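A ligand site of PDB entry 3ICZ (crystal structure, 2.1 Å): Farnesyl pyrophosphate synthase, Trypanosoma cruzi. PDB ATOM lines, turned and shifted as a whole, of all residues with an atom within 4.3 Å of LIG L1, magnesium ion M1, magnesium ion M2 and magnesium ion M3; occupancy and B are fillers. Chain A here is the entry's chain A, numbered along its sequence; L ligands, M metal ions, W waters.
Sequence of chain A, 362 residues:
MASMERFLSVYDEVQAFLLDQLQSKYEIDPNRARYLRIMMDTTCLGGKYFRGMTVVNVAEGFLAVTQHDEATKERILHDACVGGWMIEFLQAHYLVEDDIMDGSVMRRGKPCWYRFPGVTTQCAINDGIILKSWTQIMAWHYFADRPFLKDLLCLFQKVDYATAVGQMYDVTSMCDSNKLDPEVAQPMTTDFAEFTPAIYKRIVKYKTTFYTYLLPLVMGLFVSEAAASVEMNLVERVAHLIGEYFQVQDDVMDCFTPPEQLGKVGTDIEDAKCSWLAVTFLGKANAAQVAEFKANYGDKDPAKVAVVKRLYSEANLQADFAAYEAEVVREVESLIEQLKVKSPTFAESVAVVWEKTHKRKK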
ATOM      1  N   TYR A  94       6.099  -2.214  -3.438  1.00  0.00           N
ATOM      2  CA  TYR A  94       6.891  -2.136  -2.205  1.00  0.00           C
ATOM      3  C   TYR A  94       5.947  -2.321  -1.001  1.00  0.00           C
ATOM      4  O   TYR A  94       6.241  -3.071  -0.106  1.00  0.00           O
ATOM      5  CB  TYR A  94       7.595  -0.778  -2.042  1.00  0.00           C
ATOM      6  CG  TYR A  94       8.784  -0.564  -2.995  1.00  0.00           C
ATOM      7  CD1 TYR A  94       9.115   0.691  -3.451  1.00  0.00           C
ATOM      8  CD2 TYR A  94       9.584  -1.648  -3.417  1.00  0.00           C
ATOM      9  CE1 TYR A  94      10.222   0.899  -4.331  1.00  0.00           C
ATOM     10  CE2 TYR A  94      10.658  -1.453  -4.305  1.00  0.00           C
ATOM     11  CZ  TYR A  94      10.980  -0.171  -4.749  1.00  0.00           C
ATOM     12  OH  TYR A  94      12.074   0.052  -5.583  1.00  0.00           O
ATOM     13  N   LEU A  95       4.817  -1.611  -1.015  1.00  0.00           N
ATOM     14  CA  LEU A  95       3.871  -1.697   0.104  1.00  0.00           C
ATOM     15  C   LEU A  95       3.308  -3.134   0.325  1.00  0.00           C
ATOM     16  O   LEU A  95       3.199  -3.581   1.451  1.00  0.00           O
ATOM     17  CB  LEU A  95       2.756  -0.639  -0.121  1.00  0.00           C
ATOM     18  CG  LEU A  95       2.893   0.708   0.569  1.00  0.00           C
ATOM     19  CD1 LEU A  95       4.344   1.186   0.890  1.00  0.00           C
ATOM     20  CD2 LEU A  95       1.902   1.810   0.162  1.00  0.00           C
ATOM     21  N   ASP A  98       6.305  -5.236   1.730  1.00  0.00           N
ATOM     22  CA  ASP A  98       6.600  -4.692   3.100  1.00  0.00           C
ATOM     23  C   ASP A  98       5.570  -5.068   4.143  1.00  0.00           C
ATOM     24  O   ASP A  98       5.954  -5.436   5.263  1.00  0.00           O
ATOM     25  CB  ASP A  98       6.770  -3.189   3.067  1.00  0.00           C
ATOM     26  CG  ASP A  98       7.104  -2.594   4.385  1.00  0.00           C
ATOM     27  OD1 ASP A  98       8.273  -2.622   4.852  1.00  0.00           O
ATOM     28  OD2 ASP A  98       6.179  -2.010   4.967  1.00  0.00           O
ATOM     29  N   MET A 101       6.278  -8.561   5.091  1.00  0.00           N
ATOM     30  CA  MET A 101       7.520  -8.542   5.866  1.00  0.00           C
ATOM     31  C   MET A 101       7.355  -7.998   7.331  1.00  0.00           C
ATOM     32  O   MET A 101       8.026  -8.463   8.266  1.00  0.00           O
ATOM     33  CB  MET A 101       8.596  -7.776   5.077  1.00  0.00           C
ATOM     34  CG  MET A 101       9.049  -8.579   3.829  1.00  0.00           C
ATOM     35  SD  MET A 101      10.403  -7.688   2.996  1.00  0.00           S
ATOM     36  CE  MET A 101       9.715  -7.231   1.416  1.00  0.00           C
ATOM     37  N   ASP A 102       6.511  -6.974   7.485  1.00  0.00           N
ATOM     38  CA  ASP A 102       6.402  -6.251   8.766  1.00  0.00           C
ATOM     39  C   ASP A 102       5.245  -6.809   9.637  1.00  0.00           C
ATOM     40  O   ASP A 102       5.131  -6.492  10.815  1.00  0.00           O
ATOM     41  CB  ASP A 102       6.289  -4.705   8.570  1.00  0.00           C
ATOM     42  CG  ASP A 102       7.569  -4.062   7.993  1.00  0.00           C
ATOM     43  OD1 ASP A 102       8.632  -4.734   7.989  1.00  0.00           O
ATOM     44  OD2 ASP A 102       7.531  -2.874   7.528  1.00  0.00           O
ATOM     45  N   ARG A 107      -3.611  -0.898   5.858  1.00  0.00           N
ATOM     46  CA  ARG A 107      -2.919  -0.051   4.883  1.00  0.00           C
ATOM     47  C   ARG A 107      -3.970   0.849   4.154  1.00  0.00           C
ATOM     48  O   ARG A 107      -4.959   0.338   3.620  1.00  0.00           O
ATOM     49  CB  ARG A 107      -2.253  -0.925   3.835  1.00  0.00           C
ATOM     50  CG  ARG A 107      -1.509  -0.083   2.756  1.00  0.00           C
ATOM     51  CD  ARG A 107      -0.080  -0.354   3.014  1.00  0.00           C
ATOM     52  NE  ARG A 107       0.556   0.788   3.459  1.00  0.00           N
ATOM     53  CZ  ARG A 107       1.771   0.868   3.975  1.00  0.00           C
ATOM     54  NH1 ARG A 107       2.543  -0.192   4.185  1.00  0.00           N
ATOM     55  NH2 ARG A 107       2.178   2.089   4.260  1.00  0.00           N
ATOM     56  N   THR A 163      16.509   0.675  -3.121  1.00  0.00           N
ATOM     57  CA  THR A 163      15.388   0.523  -2.188  1.00  0.00           C
ATOM     58  C   THR A 163      15.405  -0.911  -1.614  1.00  0.00           C
ATOM     59  O   THR A 163      15.265  -1.111  -0.421  1.00  0.00           O
ATOM     60  CB  THR A 163      14.075   0.816  -2.897  1.00  0.00           C
ATOM     61  OG1 THR A 163      14.123   2.102  -3.487  1.00  0.00           O
ATOM     62  CG2 THR A 163      12.942   0.804  -1.953  1.00  0.00           C
ATOM     63  N   GLN A 167      15.713  -1.905   2.159  1.00  0.00           N
ATOM     64  CA  GLN A 167      14.810  -2.882   2.844  1.00  0.00           C
ATOM     65  C   GLN A 167      15.583  -3.999   3.614  1.00  0.00           C
ATOM     66  O   GLN A 167      15.179  -4.403   4.752  1.00  0.00           O
ATOM     67  CB  GLN A 167      13.795  -3.496   1.824  1.00  0.00           C
ATOM     68  CG  GLN A 167      12.714  -4.368   2.462  1.00  0.00           C
ATOM     69  CD  GLN A 167      11.657  -3.608   3.284  1.00  0.00           C
ATOM     70  OE1 GLN A 167      11.836  -2.429   3.633  1.00  0.00           O
ATOM     71  NE2 GLN A 167      10.553  -4.308   3.644  1.00  0.00           N
ATOM     72  N   ASP A 170      16.803  -2.414   6.797  1.00  0.00           N
ATOM     73  CA  ASP A 170      15.624  -2.328   7.711  1.00  0.00           C
ATOM     74  C   ASP A 170      15.252  -3.672   8.410  1.00  0.00           C
ATOM     75  O   ASP A 170      15.191  -3.810   9.622  1.00  0.00           O
ATOM     76  CB  ASP A 170      14.452  -1.727   6.910  1.00  0.00           C
ATOM     77  CG  ASP A 170      13.129  -1.650   7.736  1.00  0.00           C
ATOM     78  OD1 ASP A 170      12.703  -0.549   8.165  1.00  0.00           O
ATOM     79  OD2 ASP A 170      12.509  -2.708   7.907  1.00  0.00           O
ATOM     80  N   LYS A 207      16.253   2.795   1.751  1.00  0.00           N
ATOM     81  CA  LYS A 207      14.928   2.229   1.684  1.00  0.00           C
ATOM     82  C   LYS A 207      13.917   3.275   1.219  1.00  0.00           C
ATOM     83  O   LYS A 207      12.853   2.931   0.623  1.00  0.00           O
ATOM     84  CB  LYS A 207      14.488   1.565   3.027  1.00  0.00           C
ATOM     85  CG  LYS A 207      13.849   2.479   4.094  1.00  0.00           C
ATOM     86  CD  LYS A 207      13.152   1.688   5.215  1.00  0.00           C
ATOM     87  CE  LYS A 207      12.668   2.619   6.369  1.00  0.00           C
ATOM     88  NZ  LYS A 207      11.939   1.813   7.399  1.00  0.00           N
ATOM     89  N   THR A 208      14.187   4.554   1.490  1.00  0.00           N
ATOM     90  CA  THR A 208      13.094   5.476   1.121  1.00  0.00           C
ATOM     91  C   THR A 208      13.384   6.656   0.228  1.00  0.00           C
ATOM     92  O   THR A 208      12.559   6.994  -0.598  1.00  0.00           O
ATOM     93  CB  THR A 208      12.116   5.890   2.292  1.00  0.00           C
ATOM     94  OG1 THR A 208      12.336   7.215   2.721  1.00  0.00           O
ATOM     95  CG2 THR A 208      12.087   4.941   3.428  1.00  0.00           C
ATOM     96  N   TYR A 211      13.482   6.365  -3.897  1.00  0.00           N
ATOM     97  CA  TYR A 211      12.213   6.123  -4.666  1.00  0.00           C
ATOM     98  C   TYR A 211      11.145   7.130  -4.326  1.00  0.00           C
ATOM     99  O   TYR A 211      10.247   7.361  -5.114  1.00  0.00           O
ATOM    100  CB  TYR A 211      11.637   4.694  -4.542  1.00  0.00           C
ATOM    101  CG  TYR A 211      10.599   4.417  -3.448  1.00  0.00           C
ATOM    102  CD1 TYR A 211       9.238   4.525  -3.708  1.00  0.00           C
ATOM    103  CD2 TYR A 211      11.003   4.081  -2.160  1.00  0.00           C
ATOM    104  CE1 TYR A 211       8.297   4.243  -2.703  1.00  0.00           C
ATOM    105  CE2 TYR A 211      10.083   3.790  -1.149  1.00  0.00           C
ATOM    106  CZ  TYR A 211       8.737   3.872  -1.427  1.00  0.00           C
ATOM    107  OH  TYR A 211       7.882   3.595  -0.449  1.00  0.00           O
ATOM    108  N   GLN A 247      10.937  10.080   6.233  1.00  0.00           N
ATOM    109  CA  GLN A 247      10.954   8.830   6.966  1.00  0.00           C
ATOM    110  C   GLN A 247      10.875   9.030   8.487  1.00  0.00           C
ATOM    111  O   GLN A 247      10.318   8.173   9.211  1.00  0.00           O
ATOM    112  CB  GLN A 247      12.152   7.961   6.623  1.00  0.00           C
ATOM    113  CG  GLN A 247      12.121   6.508   7.273  1.00  0.00           C
ATOM    114  CD  GLN A 247      10.912   5.690   6.810  1.00  0.00           C
ATOM    115  OE1 GLN A 247      10.564   5.712   5.624  1.00  0.00           O
ATOM    116  NE2 GLN A 247      10.275   4.965   7.745  1.00  0.00           N
ATOM    117  N   ASP A 250       7.304   9.401   9.336  1.00  0.00           N
ATOM    118  CA  ASP A 250       6.665   8.111   9.249  1.00  0.00           C
ATOM    119  C   ASP A 250       6.873   7.368  10.558  1.00  0.00           C
ATOM    120  O   ASP A 250       5.935   6.770  11.057  1.00  0.00           O
ATOM    121  CB  ASP A 250       7.272   7.268   8.134  1.00  0.00           C
ATOM    122  CG  ASP A 250       6.533   5.964   7.944  1.00  0.00           C
ATOM    123  OD1 ASP A 250       5.286   5.999   7.700  1.00  0.00           O
ATOM    124  OD2 ASP A 250       7.192   4.897   8.054  1.00  0.00           O
ATOM    125  N   ASP A 254       3.985   6.273  13.267  1.00  0.00           N
ATOM    126  CA  ASP A 254       3.822   4.832  13.546  1.00  0.00           C
ATOM    127  C   ASP A 254       3.498   4.591  15.033  1.00  0.00           C
ATOM    128  O   ASP A 254       2.618   3.780  15.341  1.00  0.00           O
ATOM    129  CB  ASP A 254       5.082   4.038  13.192  1.00  0.00           C
ATOM    130  CG  ASP A 254       4.878   2.532  13.290  1.00  0.00           C
ATOM    131  OD1 ASP A 254       4.401   1.953  12.274  1.00  0.00           O
ATOM    132  OD2 ASP A 254       5.200   1.921  14.349  1.00  0.00           O
ATOM    133  N   LYS A 264      -2.957   3.324   8.874  1.00  0.00           N
ATOM    134  CA  LYS A 264      -2.232   2.070   9.176  1.00  0.00           C
ATOM    135  C   LYS A 264      -2.069   1.879  10.660  1.00  0.00           C
ATOM    136  O   LYS A 264      -2.233   2.837  11.440  1.00  0.00           O
ATOM    137  CB  LYS A 264      -0.861   2.000   8.455  1.00  0.00           C
ATOM    138  CG  LYS A 264       0.025   3.239   8.525  1.00  0.00           C
ATOM    139  CD  LYS A 264       1.247   3.130   7.535  1.00  0.00           C
ATOM    140  CE  LYS A 264       2.235   4.267   7.761  1.00  0.00           C
ATOM    141  NZ  LYS A 264       3.391   4.437   6.766  1.00  0.00           N
ATOM    142  N   ASP A 268       6.370  -0.827  14.503  1.00  0.00           N
ATOM    143  CA  ASP A 268       7.830  -0.643  14.641  1.00  0.00           C
ATOM    144  C   ASP A 268       8.354  -1.134  16.009  1.00  0.00           C
ATOM    145  O   ASP A 268       9.388  -1.803  16.076  1.00  0.00           O
ATOM    146  CB  ASP A 268       8.249   0.781  14.403  1.00  0.00           C
ATOM    147  CG  ASP A 268       8.132   1.198  12.945  1.00  0.00           C
ATOM    148  OD1 ASP A 268       7.905   0.316  12.057  1.00  0.00           O
ATOM    149  OD2 ASP A 268       8.232   2.437  12.712  1.00  0.00           O
ATOM    150  N   LYS A 273      12.050  -2.477  15.392  1.00  0.00           N
ATOM    151  CA  LYS A 273      12.728  -1.684  14.352  1.00  0.00           C
ATOM    152  C   LYS A 273      13.698  -0.633  14.901  1.00  0.00           C
ATOM    153  O   LYS A 273      13.423  -0.038  15.937  1.00  0.00           O
ATOM    154  CB  LYS A 273      11.679  -1.017  13.415  1.00  0.00           C
ATOM    155  CG  LYS A 273      10.921  -2.085  12.577  1.00  0.00           C
ATOM    156  CD  LYS A 273      11.900  -2.715  11.598  1.00  0.00           C
ATOM    157  CE  LYS A 273      11.300  -3.889  10.858  1.00  0.00           C
ATOM    158  NZ  LYS A 273       9.947  -3.641  10.244  1.00  0.00           N
HETATM  159  C1  LIG L   1       6.907   1.178   4.223  1.00  0.00           C
HETATM  160  C2  LIG L   1       6.949   1.912   5.585  1.00  0.00           C
HETATM  161  P1  LIG L   1       5.263   1.772   6.253  1.00  0.00           P
HETATM  162  O1  LIG L   1       4.337   2.425   5.280  1.00  0.00           O
HETATM  163  O2  LIG L   1       5.254   2.541   7.570  1.00  0.00           O
HETATM  164  N1  LIG L   1       8.176   1.298   3.419  1.00  0.00           N
HETATM  165  O3  LIG L   1       5.054   0.328   6.457  1.00  0.00           O
HETATM  166  C3  LIG L   1       9.046   2.372   3.444  1.00  0.00           C
HETATM  167  C4  LIG L   1      10.215   2.308   2.665  1.00  0.00           C
HETATM  168  P2  LIG L   1       8.204   1.195   6.721  1.00  0.00           P
HETATM  169  C5  LIG L   1      10.488   1.171   1.850  1.00  0.00           C
HETATM  170  O4  LIG L   1       7.959  -0.290   6.681  1.00  0.00           O
HETATM  171  C6  LIG L   1       9.561   0.099   1.854  1.00  0.00           C
HETATM  172  O5  LIG L   1       9.577   1.382   6.145  1.00  0.00           O
HETATM  173  C7  LIG L   1       8.455   0.228   2.678  1.00  0.00           C
HETATM  174  O6  LIG L   1       8.081   1.986   8.026  1.00  0.00           O
HETATM  175  C8  LIG L   1       9.671  -1.219   1.129  1.00  0.00           C
HETATM  176  C9  LIG L   1      10.693  -1.491   0.340  1.00  0.00           C
HETATM  177  C10 LIG L   1      10.909  -2.774  -0.458  1.00  0.00           C
HETATM  178  C11 LIG L   1       9.841  -3.818  -0.234  1.00  0.00           C
HETATM  179  C1  LG2 L   2       4.582   4.920   2.911  1.00  0.00           C
HETATM  180  O1  LG2 L   2       4.638   6.019   2.012  1.00  0.00           O
HETATM  181  C2  LG2 L   2       5.959   4.243   2.921  1.00  0.00           C
HETATM  182  C3  LG2 L   2       7.077   5.187   3.344  1.00  0.00           C
HETATM  183  C4  LG2 L   2       7.129   5.814   4.527  1.00  0.00           C
HETATM  184  C5  LG2 L   2       8.167   5.403   2.320  1.00  0.00           C
HETATM  185  P1  LG2 L   2       3.384   7.055   1.957  1.00  0.00           P
HETATM  186  O2  LG2 L   2       3.100   7.458   3.351  1.00  0.00           O
HETATM  187  O3  LG2 L   2       3.653   8.066   0.858  1.00  0.00           O
HETATM  188  O4  LG2 L   2       2.132   6.128   1.460  1.00  0.00           O
HETATM  189  P2  LG2 L   2       0.912   6.497   0.444  1.00  0.00           P
HETATM  190  O5  LG2 L   2       1.325   5.957  -0.929  1.00  0.00           O
HETATM  191  O6  LG2 L   2       0.649   7.929   0.507  1.00  0.00           O
HETATM  192  O7  LG2 L   2      -0.184   5.738   1.143  1.00  0.00           O
HETATM  193 MG    MG M   1       6.014  -1.330   6.939  1.00  0.00          MG
HETATM  194 MG    MG M   2       6.606   3.162   8.857  1.00  0.00          MG
HETATM  195 MG    MG M   3       9.120  -1.976   6.577  1.00  0.00          MG
HETATM  196  O   HOH W   1       8.048   3.518  10.430  1.00  0.00           O
HETATM  197  O   HOH W   2       2.855   0.240   8.359  1.00  0.00           O
HETATM  198  O   HOH W   3       5.111   4.229  10.019  1.00  0.00           O
HETATM  199  O   HOH W   4       5.964  -1.138   9.030  1.00  0.00           O
HETATM  200  O   HOH W   5       4.367  -2.548   7.039  1.00  0.00           O
HETATM  201  O   HOH W   6      10.089  -1.575   8.326  1.00  0.00           O
HETATM  202  O   HOH W   7       9.544   0.733   9.920  1.00  0.00           O
HETATM  203  O   HOH W   8      10.573  -1.044   5.537  1.00  0.00           O
HETATM  204  O   HOH W   9      10.200  -3.636   6.580  1.00  0.00           O
HETATM  205  O   HOH W  10       6.334   1.561  10.210  1.00  0.00           O
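NH2 of Arg 107 lies within salt-bridge range of O1 of LIG L1 (2.4 Å).
The side-chain amino group (NZ) of Lys 264 is in salt-bridge range of an oxygen (O1) of LIG L1 (2.7 Å).
O5 of LIG L1 is in salt-bridge range of NZ of Lys 207, 2.7 Å away.
The side-chain carboxylate (OD1) of Asp 250 lies within salt-bridge range of the side-chain amino group (NZ) of Lys 264, at 2.6 Å.
NE2 of Gln 247 lies close to OD2 of Asp 250 (3.1 Å).
OD1 of Asp 98 sits close to NE2 of Gln 167 (3.1 Å).
OD1 of Asp 102 lies within salt-bridge range of NZ of Lys 273 (2.8 Å).
The side-chain amino group of Lys 207 is in salt-bridge range of the side-chain carboxylate of Asp 170, 2.6 Å away.
NE2 of Gln 167 lies within hydrogen-bond range of SD of Met 101, at 3.4 Å.
OD2 of Asp 170 lies within salt-bridge range of NZ of Lys 273.
Residues that only touch LIG L1: Thr 208 (3.3 Å), Tyr 94 (3.4 Å), Gln 167 (3.5 Å), Gln 247 (3.7 Å), Met 101 (3.8 Å) and Thr 163 (3.9 Å).
Hydrophobic or aromatic side chains that line LIG L1: Tyr 94 and Met 101.
Of the 18 residues printed, 12 come within 4 Å of LIG L1.
The nearest printed residue that does not touch LIG L1 is Tyr 211 (4.002 Å).
The nearest printed residue that does not touch magnesium ion M1 is Arg 107 (4.6 Å).
One residue has an atom within 4 Å of magnesium ion M2: Asp 250.
The nearest printed residue that does not touch magnesium ion M2 is Lys 264 (4.04 Å).
Residues that only touch magnesium ion M3: Asp 170.
Three residues have an atom within 4 Å of magnesium ion M3: Asp 98, Asp 102 and Asp 170.
Magnesium ion M1 is bound by O3 of LIG L1.
Water W5 binds magnesium ion M1, at 2.1 Å.
Magnesium ion M1 is bound by OD2 of Asp 98 (2.1 Å).
Magnesium ion M1 is bound by water W4.
O4 of LIG L1 is bound to magnesium ion M1 (2.2 Å).
The side-chain carboxylate (OD2) of Asp 102 binds magnesium ion M1 (2.2 Å).
Magnesium ion M1 has six donor atoms within binding distance.
Magnesium ion M2 is bound by O2 of LIG L1 (2.0 Å).
The side-chain carboxylate (OD2) of Asp 250 is bound to magnesium ion M2 (2.0 Å).
O6 of LIG L1 binds magnesium ion M2.
Magnesium ion M2 is bound by water W10.
Water W1 binds magnesium ion M2 (2.2 Å).
Water W3 is bound to magnesium ion M2.
Magnesium ion M3 is bound by water W9 (2.0 Å), water W8 (2.0 Å), the side-chain carboxylate (OD1) of Asp 98 (2.0 Å), water W6 (2.0 Å), an oxygen (O4) of LIG L1 (2.0 Å) and the side-chain carboxylate (OD2) of Asp 102 (2.1 Å).
Water W3 bridges the backbone carbonyl oxygen (O) of Asp 250 (2.9 Å) and the side-chain carboxylate (OD1) of Asp 254 (3.3 Å).
Water W10 lies within hydrogen-bond range of OD1 of Asp 268 and OD1 of Asp 254.
Water W6 lies within hydrogen-bond range of the side-chain carboxylate of Asp 170 (2.7 Å), the side-chain amino group of Lys 273 (2.8 Å) and the side-chain carboxylate of Asp 102 (3.5 Å).
Water W8 lies within hydrogen-bond range of the side-chain amide oxygen of Gln 167, an oxygen (O5) of LIG L1 and the side-chain carboxylate of Asp 170.
Water W9 bridges OD2 of Asp 170 and NE2 of Gln 167.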
